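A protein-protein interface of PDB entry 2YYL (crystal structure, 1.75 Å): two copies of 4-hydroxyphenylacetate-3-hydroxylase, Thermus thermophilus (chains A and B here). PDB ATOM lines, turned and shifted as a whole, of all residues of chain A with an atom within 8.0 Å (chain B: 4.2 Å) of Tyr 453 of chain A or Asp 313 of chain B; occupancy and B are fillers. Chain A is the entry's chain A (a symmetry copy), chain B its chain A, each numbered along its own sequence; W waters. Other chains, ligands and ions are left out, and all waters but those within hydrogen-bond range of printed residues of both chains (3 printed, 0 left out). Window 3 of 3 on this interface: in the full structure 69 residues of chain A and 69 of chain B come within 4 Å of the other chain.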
ATOM      1  N   ASP A 359      -0.286  22.887  -1.631  1.00  0.00           N
ATOM      2  CA  ASP A 359      -0.712  22.552  -2.990  1.00  0.00           C
ATOM      3  C   ASP A 359      -1.764  21.448  -2.856  1.00  0.00           C
ATOM      4  O   ASP A 359      -2.707  21.364  -3.643  1.00  0.00           O
ATOM      5  CB  ASP A 359       0.466  22.048  -3.837  1.00  0.00           C
ATOM      6  CG  ASP A 359       1.209  23.176  -4.541  1.00  0.00           C
ATOM      7  OD1 ASP A 359       0.732  24.329  -4.491  1.00  0.00           O
ATOM      8  OD2 ASP A 359       2.266  22.907  -5.156  1.00  0.00           O
ATOM      9  N   ASN A 363      -5.705  22.303  -4.064  1.00  0.00           N
ATOM     10  CA  ASN A 363      -6.123  21.540  -5.229  1.00  0.00           C
ATOM     11  C   ASN A 363      -7.162  20.494  -4.854  1.00  0.00           C
ATOM     12  O   ASN A 363      -7.839  19.937  -5.720  1.00  0.00           O
ATOM     13  CB  ASN A 363      -4.917  20.896  -5.908  1.00  0.00           C
ATOM     14  CG  ASN A 363      -4.172  21.878  -6.779  1.00  0.00           C
ATOM     15  OD1 ASN A 363      -4.730  22.399  -7.738  1.00  0.00           O
ATOM     16  ND2 ASN A 363      -2.917  22.152  -6.442  1.00  0.00           N
ATOM     17  N   ARG A 447      -5.381  23.718 -15.228  1.00  0.00           N
ATOM     18  CA  ARG A 447      -4.019  24.203 -15.267  1.00  0.00           C
ATOM     19  C   ARG A 447      -3.299  24.121 -13.929  1.00  0.00           C
ATOM     20  O   ARG A 447      -2.075  23.976 -13.891  1.00  0.00           O
ATOM     21  CB  ARG A 447      -4.001  25.614 -15.844  1.00  0.00           C
ATOM     22  CG  ARG A 447      -4.079  25.553 -17.367  1.00  0.00           C
ATOM     23  CD  ARG A 447      -4.457  26.867 -17.987  1.00  0.00           C
ATOM     24  NE  ARG A 447      -5.878  27.141 -17.815  1.00  0.00           N
ATOM     25  CZ  ARG A 447      -6.472  28.238 -18.265  1.00  0.00           C
ATOM     26  NH1 ARG A 447      -5.761  29.154 -18.908  1.00  0.00           N
ATOM     27  NH2 ARG A 447      -7.770  28.422 -18.070  1.00  0.00           N
ATOM     28  N   MET A 448      -4.048  24.200 -12.832  1.00  0.00           N
ATOM     29  CA  MET A 448      -3.432  24.086 -11.515  1.00  0.00           C
ATOM     30  C   MET A 448      -2.868  22.679 -11.353  1.00  0.00           C
ATOM     31  O   MET A 448      -1.787  22.494 -10.792  1.00  0.00           O
ATOM     32  CB  MET A 448      -4.457  24.356 -10.411  1.00  0.00           C
ATOM     33  CG  MET A 448      -4.801  25.826 -10.263  1.00  0.00           C
ATOM     34  SD  MET A 448      -6.033  26.105  -8.988  1.00  0.00           S
ATOM     35  CE  MET A 448      -5.090  25.707  -7.499  1.00  0.00           C
ATOM     36  N   TYR A 449      -3.603  21.683 -11.841  1.00  0.00           N
ATOM     37  CA  TYR A 449      -3.140  20.306 -11.735  1.00  0.00           C
ATOM     38  C   TYR A 449      -1.955  20.059 -12.661  1.00  0.00           C
ATOM     39  O   TYR A 449      -1.028  19.321 -12.315  1.00  0.00           O
ATOM     40  CB  TYR A 449      -4.281  19.326 -12.034  1.00  0.00           C
ATOM     41  CG  TYR A 449      -5.076  18.949 -10.797  1.00  0.00           C
ATOM     42  CD1 TYR A 449      -5.750  19.918 -10.049  1.00  0.00           C
ATOM     43  CD2 TYR A 449      -5.120  17.625 -10.353  1.00  0.00           C
ATOM     44  CE1 TYR A 449      -6.447  19.576  -8.886  1.00  0.00           C
ATOM     45  CE2 TYR A 449      -5.809  17.275  -9.194  1.00  0.00           C
ATOM     46  CZ  TYR A 449      -6.469  18.252  -8.466  1.00  0.00           C
ATOM     47  OH  TYR A 449      -7.133  17.894  -7.315  1.00  0.00           O
ATOM     48  N   GLN A 450      -1.974  20.675 -13.841  1.00  0.00           N
ATOM     49  CA  GLN A 450      -0.855  20.512 -14.760  1.00  0.00           C
ATOM     50  C   GLN A 450       0.379  21.185 -14.155  1.00  0.00           C
ATOM     51  O   GLN A 450       1.499  20.692 -14.292  1.00  0.00           O
ATOM     52  CB  GLN A 450      -1.203  21.116 -16.124  1.00  0.00           C
ATOM     53  CG  GLN A 450      -2.123  20.221 -16.928  1.00  0.00           C
ATOM     54  CD  GLN A 450      -2.604  20.856 -18.214  1.00  0.00           C
ATOM     55  OE1 GLN A 450      -1.910  21.672 -18.816  1.00  0.00           O
ATOM     56  NE2 GLN A 450      -3.792  20.462 -18.659  1.00  0.00           N
ATOM     57  N   THR A 451       0.167  22.305 -13.471  1.00  0.00           N
ATOM     58  CA  THR A 451       1.265  23.017 -12.826  1.00  0.00           C
ATOM     59  C   THR A 451       1.860  22.156 -11.709  1.00  0.00           C
ATOM     60  O   THR A 451       3.080  22.049 -11.582  1.00  0.00           O
ATOM     61  CB  THR A 451       0.784  24.371 -12.237  1.00  0.00           C
ATOM     62  OG1 THR A 451       0.471  25.274 -13.310  1.00  0.00           O
ATOM     63  CG2 THR A 451       1.860  24.992 -11.359  1.00  0.00           C
ATOM     64  N   LEU A 452       0.999  21.540 -10.905  1.00  0.00           N
ATOM     65  CA  LEU A 452       1.465  20.691  -9.811  1.00  0.00           C
ATOM     66  C   LEU A 452       2.295  19.532 -10.360  1.00  0.00           C
ATOM     67  O   LEU A 452       3.343  19.192  -9.816  1.00  0.00           O
ATOM     68  CB  LEU A 452       0.274  20.159  -8.999  1.00  0.00           C
ATOM     69  CG  LEU A 452       0.595  19.146  -7.890  1.00  0.00           C
ATOM     70  CD1 LEU A 452       1.634  19.737  -6.947  1.00  0.00           C
ATOM     71  CD2 LEU A 452      -0.682  18.776  -7.119  1.00  0.00           C
ATOM     72  N   TYR A 453       1.826  18.923 -11.442  1.00  0.00           N
ATOM     73  CA  TYR A 453       2.559  17.821 -12.047  1.00  0.00           C
ATOM     74  C   TYR A 453       3.975  18.261 -12.426  1.00  0.00           C
ATOM     75  O   TYR A 453       4.954  17.571 -12.140  1.00  0.00           O
ATOM     76  CB  TYR A 453       1.853  17.337 -13.312  1.00  0.00           C
ATOM     77  CG  TYR A 453       2.704  16.388 -14.122  1.00  0.00           C
ATOM     78  CD1 TYR A 453       2.841  15.053 -13.745  1.00  0.00           C
ATOM     79  CD2 TYR A 453       3.423  16.840 -15.230  1.00  0.00           C
ATOM     80  CE1 TYR A 453       3.680  14.186 -14.451  1.00  0.00           C
ATOM     81  CE2 TYR A 453       4.263  15.983 -15.940  1.00  0.00           C
ATOM     82  CZ  TYR A 453       4.386  14.661 -15.544  1.00  0.00           C
ATOM     83  OH  TYR A 453       5.216  13.811 -16.246  1.00  0.00           O
ATOM     84  N   ASN A 454       4.075  19.417 -13.067  1.00  0.00           N
ATOM     85  CA  ASN A 454       5.370  19.906 -13.504  1.00  0.00           C
ATOM     86  C   ASN A 454       6.316  20.403 -12.411  1.00  0.00           C
ATOM     87  O   ASN A 454       7.534  20.272 -12.552  1.00  0.00           O
ATOM     88  CB  ASN A 454       5.176  20.974 -14.585  1.00  0.00           C
ATOM     89  CG  ASN A 454       4.583  20.399 -15.866  1.00  0.00           C
ATOM     90  OD1 ASN A 454       3.405  20.601 -16.173  1.00  0.00           O
ATOM     91  ND2 ASN A 454       5.397  19.664 -16.610  1.00  0.00           N
ATOM     92  N   VAL A 455       5.791  20.947 -11.317  1.00  0.00           N
ATOM     93  CA  VAL A 455       6.681  21.439 -10.261  1.00  0.00           C
ATOM     94  C   VAL A 455       7.064  20.401  -9.219  1.00  0.00           C
ATOM     95  O   VAL A 455       8.113  20.509  -8.587  1.00  0.00           O
ATOM     96  CB  VAL A 455       6.079  22.640  -9.489  1.00  0.00           C
ATOM     97  CG1 VAL A 455       5.728  23.753 -10.443  1.00  0.00           C
ATOM     98  CG2 VAL A 455       4.867  22.201  -8.694  1.00  0.00           C
ATOM     99  N   TYR A 456       6.217  19.397  -9.036  1.00  0.00           N
ATOM    100  CA  TYR A 456       6.467  18.379  -8.024  1.00  0.00           C
ATOM    101  C   TYR A 456       7.666  17.497  -8.332  1.00  0.00           C
ATOM    102  O   TYR A 456       7.876  17.110  -9.478  1.00  0.00           O
ATOM    103  CB  TYR A 456       5.228  17.497  -7.864  1.00  0.00           C
ATOM    104  CG  TYR A 456       5.142  16.816  -6.517  1.00  0.00           C
ATOM    105  CD1 TYR A 456       4.806  17.539  -5.375  1.00  0.00           C
ATOM    106  CD2 TYR A 456       5.376  15.448  -6.390  1.00  0.00           C
ATOM    107  CE1 TYR A 456       4.697  16.914  -4.132  1.00  0.00           C
ATOM    108  CE2 TYR A 456       5.273  14.813  -5.155  1.00  0.00           C
ATOM    109  CZ  TYR A 456       4.929  15.550  -4.032  1.00  0.00           C
ATOM    110  OH  TYR A 456       4.785  14.910  -2.822  1.00  0.00           O
ATOM    111  N   ASN A 457       8.453  17.187  -7.305  1.00  0.00           N
ATOM    112  CA  ASN A 457       9.609  16.316  -7.483  1.00  0.00           C
ATOM    113  C   ASN A 457       9.133  14.868  -7.422  1.00  0.00           C
ATOM    114  O   ASN A 457       8.912  14.319  -6.342  1.00  0.00           O
ATOM    115  CB  ASN A 457      10.652  16.562  -6.394  1.00  0.00           C
ATOM    116  CG  ASN A 457      11.840  15.630  -6.518  1.00  0.00           C
ATOM    117  OD1 ASN A 457      12.041  14.998  -7.561  1.00  0.00           O
ATOM    118  ND2 ASN A 457      12.642  15.546  -5.461  1.00  0.00           N
ATOM    119  N   LYS A 458       8.981  14.261  -8.593  1.00  0.00           N
ATOM    120  CA  LYS A 458       8.506  12.888  -8.710  1.00  0.00           C
ATOM    121  C   LYS A 458       9.632  11.859  -8.723  1.00  0.00           C
ATOM    122  O   LYS A 458       9.384  10.657  -8.668  1.00  0.00           O
ATOM    123  CB  LYS A 458       7.677  12.757  -9.994  1.00  0.00           C
ATOM    124  CG  LYS A 458       6.488  13.714 -10.050  1.00  0.00           C
ATOM    125  CD  LYS A 458       5.886  13.832 -11.452  1.00  0.00           C
ATOM    126  CE  LYS A 458       6.823  14.545 -12.429  1.00  0.00           C
ATOM    127  NZ  LYS A 458       7.121  15.956 -12.035  1.00  0.00           N
ATOM    128  N   GLU A 459      10.872  12.333  -8.771  1.00  0.00           N
ATOM    129  CA  GLU A 459      12.023  11.438  -8.843  1.00  0.00           C
ATOM    130  C   GLU A 459      12.199  10.378  -7.755  1.00  0.00           C
ATOM    131  O   GLU A 459      12.505   9.232  -8.064  1.00  0.00           O
ATOM    132  CB  GLU A 459      13.303  12.267  -8.973  1.00  0.00           C
ATOM    133  CG  GLU A 459      13.291  13.173 -10.193  1.00  0.00           C
ATOM    134  CD  GLU A 459      12.809  12.461 -11.446  1.00  0.00           C
ATOM    135  OE1 GLU A 459      13.413  11.431 -11.824  1.00  0.00           O
ATOM    136  OE2 GLU A 459      11.822  12.930 -12.056  1.00  0.00           O
ATOM    137  N   LYS A 462       9.919   7.420  -8.515  1.00  0.00           N
ATOM    138  CA  LYS A 462      10.290   6.686  -9.714  1.00  0.00           C
ATOM    139  C   LYS A 462      11.536   5.860  -9.409  1.00  0.00           C
ATOM    140  O   LYS A 462      11.666   4.728  -9.871  1.00  0.00           O
ATOM    141  CB  LYS A 462      10.559   7.649 -10.874  1.00  0.00           C
ATOM    142  CG  LYS A 462       9.318   8.422 -11.307  1.00  0.00           C
ATOM    143  CD  LYS A 462       9.523   9.165 -12.620  1.00  0.00           C
ATOM    144  CE  LYS A 462      10.555  10.262 -12.505  1.00  0.00           C
ATOM    145  NZ  LYS A 462      10.719  10.974 -13.810  1.00  0.00           N
ATOM    146  N   ALA B 307       3.598   6.700 -17.707  1.00  0.00           N
ATOM    147  CA  ALA B 307       3.330   7.850 -18.564  1.00  0.00           C
ATOM    148  C   ALA B 307       4.575   8.300 -19.322  1.00  0.00           C
ATOM    149  O   ALA B 307       4.523   8.572 -20.519  1.00  0.00           O
ATOM    150  CB  ALA B 307       2.772   9.003 -17.734  1.00  0.00           C
ATOM    151  N   GLU B 308       5.698   8.372 -18.620  1.00  0.00           N
ATOM    152  CA  GLU B 308       6.948   8.786 -19.240  1.00  0.00           C
ATOM    153  C   GLU B 308       7.386   7.716 -20.239  1.00  0.00           C
ATOM    154  O   GLU B 308       7.816   8.020 -21.359  1.00  0.00           O
ATOM    155  CB  GLU B 308       8.008   8.964 -18.152  1.00  0.00           C
ATOM    156  CG  GLU B 308       9.347   9.493 -18.624  1.00  0.00           C
ATOM    157  CD  GLU B 308      10.313   9.693 -17.468  1.00  0.00           C
ATOM    158  OE1 GLU B 308      10.766   8.687 -16.886  1.00  0.00           O
ATOM    159  OE2 GLU B 308      10.608  10.857 -17.133  1.00  0.00           O
ATOM    160  N   GLY B 311       5.384   7.864 -23.489  1.00  0.00           N
ATOM    161  CA  GLY B 311       5.210   9.209 -24.010  1.00  0.00           C
ATOM    162  C   GLY B 311       3.837   9.821 -23.789  1.00  0.00           C
ATOM    163  O   GLY B 311       3.462  10.779 -24.464  1.00  0.00           O
ATOM    164  N   ALA B 312       3.083   9.281 -22.841  1.00  0.00           N
ATOM    165  CA  ALA B 312       1.751   9.802 -22.564  1.00  0.00           C
ATOM    166  C   ALA B 312       1.796  11.029 -21.658  1.00  0.00           C
ATOM    167  O   ALA B 312       0.799  11.740 -21.520  1.00  0.00           O
ATOM    168  CB  ALA B 312       0.887   8.713 -21.933  1.00  0.00           C
ATOM    169  N   ASP B 313       2.959  11.281 -21.059  1.00  0.00           N
ATOM    170  CA  ASP B 313       3.136  12.411 -20.152  1.00  0.00           C
ATOM    171  C   ASP B 313       3.019  13.780 -20.825  1.00  0.00           C
ATOM    172  O   ASP B 313       2.916  14.803 -20.147  1.00  0.00           O
ATOM    173  CB  ASP B 313       4.490  12.302 -19.439  1.00  0.00           C
ATOM    174  CG  ASP B 313       5.666  12.356 -20.405  1.00  0.00           C
ATOM    175  OD1 ASP B 313       5.621  11.668 -21.447  1.00  0.00           O
ATOM    176  OD2 ASP B 313       6.643  13.076 -20.119  1.00  0.00           O
ATOM    177  N   VAL B 314       3.033  13.810 -22.155  1.00  0.00           N
ATOM    178  CA  VAL B 314       2.922  15.083 -22.859  1.00  0.00           C
ATOM    179  C   VAL B 314       1.480  15.574 -22.895  1.00  0.00           C
ATOM    180  O   VAL B 314       1.219  16.741 -23.195  1.00  0.00           O
ATOM    181  CB  VAL B 314       3.444  14.981 -24.313  1.00  0.00           C
ATOM    182  CG1 VAL B 314       4.908  14.569 -24.307  1.00  0.00           C
ATOM    183  CG2 VAL B 314       2.604  13.993 -25.106  1.00  0.00           C
ATOM    184  N   TYR B 315       0.544  14.684 -22.581  1.00  0.00           N
ATOM    185  CA  TYR B 315      -0.868  15.036 -22.596  1.00  0.00           C
ATOM    186  C   TYR B 315      -1.339  15.617 -21.272  1.00  0.00           C
ATOM    187  O   TYR B 315      -1.120  15.038 -20.211  1.00  0.00           O
ATOM    188  CB  TYR B 315      -1.697  13.810 -22.977  1.00  0.00           C
ATOM    189  CG  TYR B 315      -1.369  13.345 -24.374  1.00  0.00           C
ATOM    190  CD1 TYR B 315      -1.697  14.132 -25.476  1.00  0.00           C
ATOM    191  CD2 TYR B 315      -0.646  12.176 -24.592  1.00  0.00           C
ATOM    192  CE1 TYR B 315      -1.304  13.775 -26.762  1.00  0.00           C
ATOM    193  CE2 TYR B 315      -0.243  11.806 -25.879  1.00  0.00           C
ATOM    194  CZ  TYR B 315      -0.577  12.615 -26.957  1.00  0.00           C
ATOM    195  OH  TYR B 315      -0.166  12.286 -28.230  1.00  0.00           O
ATOM    196  N   GLN B 319      -1.149  14.340 -17.159  1.00  0.00           N
ATOM    197  CA  GLN B 319      -0.423  15.072 -16.131  1.00  0.00           C
ATOM    198  C   GLN B 319      -1.368  15.341 -14.958  1.00  0.00           C
ATOM    199  O   GLN B 319      -0.977  15.235 -13.793  1.00  0.00           O
ATOM    200  CB  GLN B 319       0.098  16.397 -16.695  1.00  0.00           C
ATOM    201  CG  GLN B 319       1.009  16.235 -17.913  1.00  0.00           C
ATOM    202  CD  GLN B 319       1.531  17.558 -18.433  1.00  0.00           C
ATOM    203  OE1 GLN B 319       1.134  18.623 -17.965  1.00  0.00           O
ATOM    204  NE2 GLN B 319       2.427  17.496 -19.415  1.00  0.00           N
ATOM    205  N   ILE B 322      -1.834  12.270 -12.753  1.00  0.00           N
ATOM    206  CA  ILE B 322      -0.688  12.032 -11.891  1.00  0.00           C
ATOM    207  C   ILE B 322      -0.708  13.044 -10.743  1.00  0.00           C
ATOM    208  O   ILE B 322      -0.422  12.702  -9.595  1.00  0.00           O
ATOM    209  CB  ILE B 322       0.623  12.109 -12.700  1.00  0.00           C
ATOM    210  CG1 ILE B 322       0.664  10.927 -13.678  1.00  0.00           C
ATOM    211  CG2 ILE B 322       1.825  12.085 -11.767  1.00  0.00           C
ATOM    212  CD1 ILE B 322       1.766  10.995 -14.722  1.00  0.00           C
ATOM    213  N   ALA B 323      -1.081  14.284 -11.051  1.00  0.00           N
ATOM    214  CA  ALA B 323      -1.161  15.321 -10.027  1.00  0.00           C
ATOM    215  C   ALA B 323      -2.230  14.951  -8.994  1.00  0.00           C
ATOM    216  O   ALA B 323      -2.121  15.305  -7.823  1.00  0.00           O
ATOM    217  CB  ALA B 323      -1.488  16.668 -10.668  1.00  0.00           C
HETATM  218  O   HOH W   1       4.738  19.513 -19.288  1.00  0.00           O
HETATM  219  O   HOH W   2       0.993  20.802 -19.414  1.00  0.00           O
HETATM  220  O   HOH W   3       6.973  14.893 -18.168  1.00  0.00           O
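Of the 16 printed residues of chain A, 6 touch a printed residue of chain B.
Hydrophobic or aromatic side chains of chain B that line the printed part of chain A: Ile 322 and Ala 323.
Among the printed residues, 8 pairs touch across the chains.
OE2 of Glu 308 of chain B is in salt-bridge range of NZ of Lys 462 of chain A (3.3 Å).
Water W2 lies within hydrogen-bond range of OE1 of Gln 319 of chain B and OE1 of Gln 450 of chain A.
Water W3 lies within hydrogen-bond range of the side-chain carboxylate of Asp 313 of chain B (2.7 Å) and the side-chain hydroxyl of Tyr 453 of chain A (2.8 Å).
Water W1 lies within hydrogen-bond range of ND2 of Asn 454 of chain A and NE2 of Gln 319 of chain B.
CB of Ala 323 of chain B touches O of Tyr 449 of chain A, 3.2 Å away.
CG of Gln 450 of chain A touches OE1 of Gln 319 of chain B, 3.8 Å away.
Ala 323 of chain B touches Leu 452 of chain A.
Asp 313 of chain B touches Tyr 453 of chain A (CB to OH, 3.6 Å).
Gln 319 of chain B touches Tyr 453 of chain A (O to CB, 3.6 Å).
Tyr 453 of chain A touches Ile 322 of chain B (CD1 to CG2, 3.7 Å).
Gln 319 of chain B touches Asn 454 of chain A (OE1 to OD1, 3.5 Å).
O of Asp 313 of chain B is in hydrogen-bond range of NE2 of Gln 319 of chain B (2.8 Å).
The side-chain amino group (NZ) of Lys 458 of chain A lies within hydrogen-bond range of the backbone carbonyl oxygen (O) of Tyr 453 of chain A.
The backbone carbonyl oxygen (O) of Ala 307 of chain B lies within hydrogen-bond range of the backbone NH (N) of Asp 313 of chain B (3.2 Å).
The side-chain carboxylate (OE2) of Glu 459 of chain A is in salt-bridge range of the side-chain amino group (NZ) of Lys 462 of chain A.
O of Asn 363 of chain A sits at hydrogen-bond distance from OH of Tyr 449 of chain A (2.7 Å).
The side-chain amide oxygen (OD1) of Asn 454 of chain A sits close to the backbone carbonyl oxygen (O) of Gln 450 of chain A (2.7 Å).
Of the printed residues of chain B, Tyr 449 of chain A touches Ala 323.
Of chain B, only Asp 313 (3.6 Å), Gln 319 (3.6 Å) and Ile 322 (3.7 Å) come within 4 Å of Tyr 453 of chain A.
Printed residues of chain B within 4 Å of Lys 462 of chain A: Glu 308.
No residue of chain A comes within 4 Å of Ala 312 of chain B.
Asp 313 of chain B touches just one residue of chain A: Tyr 453 (3.6 Å).
Printed residues of chain A within 4 Å of Ile 322 of chain B: Tyr 453 (3.7 Å).
The nearest printed residue of chain A that does not touch Ala 323 of chain B is Tyr 453 of chain A (4.1 Å).
No position is printed for both chains.
Of the 8 pairs that touch across the chains among the printed residues, none has its exchanged pair printed and touching as well.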
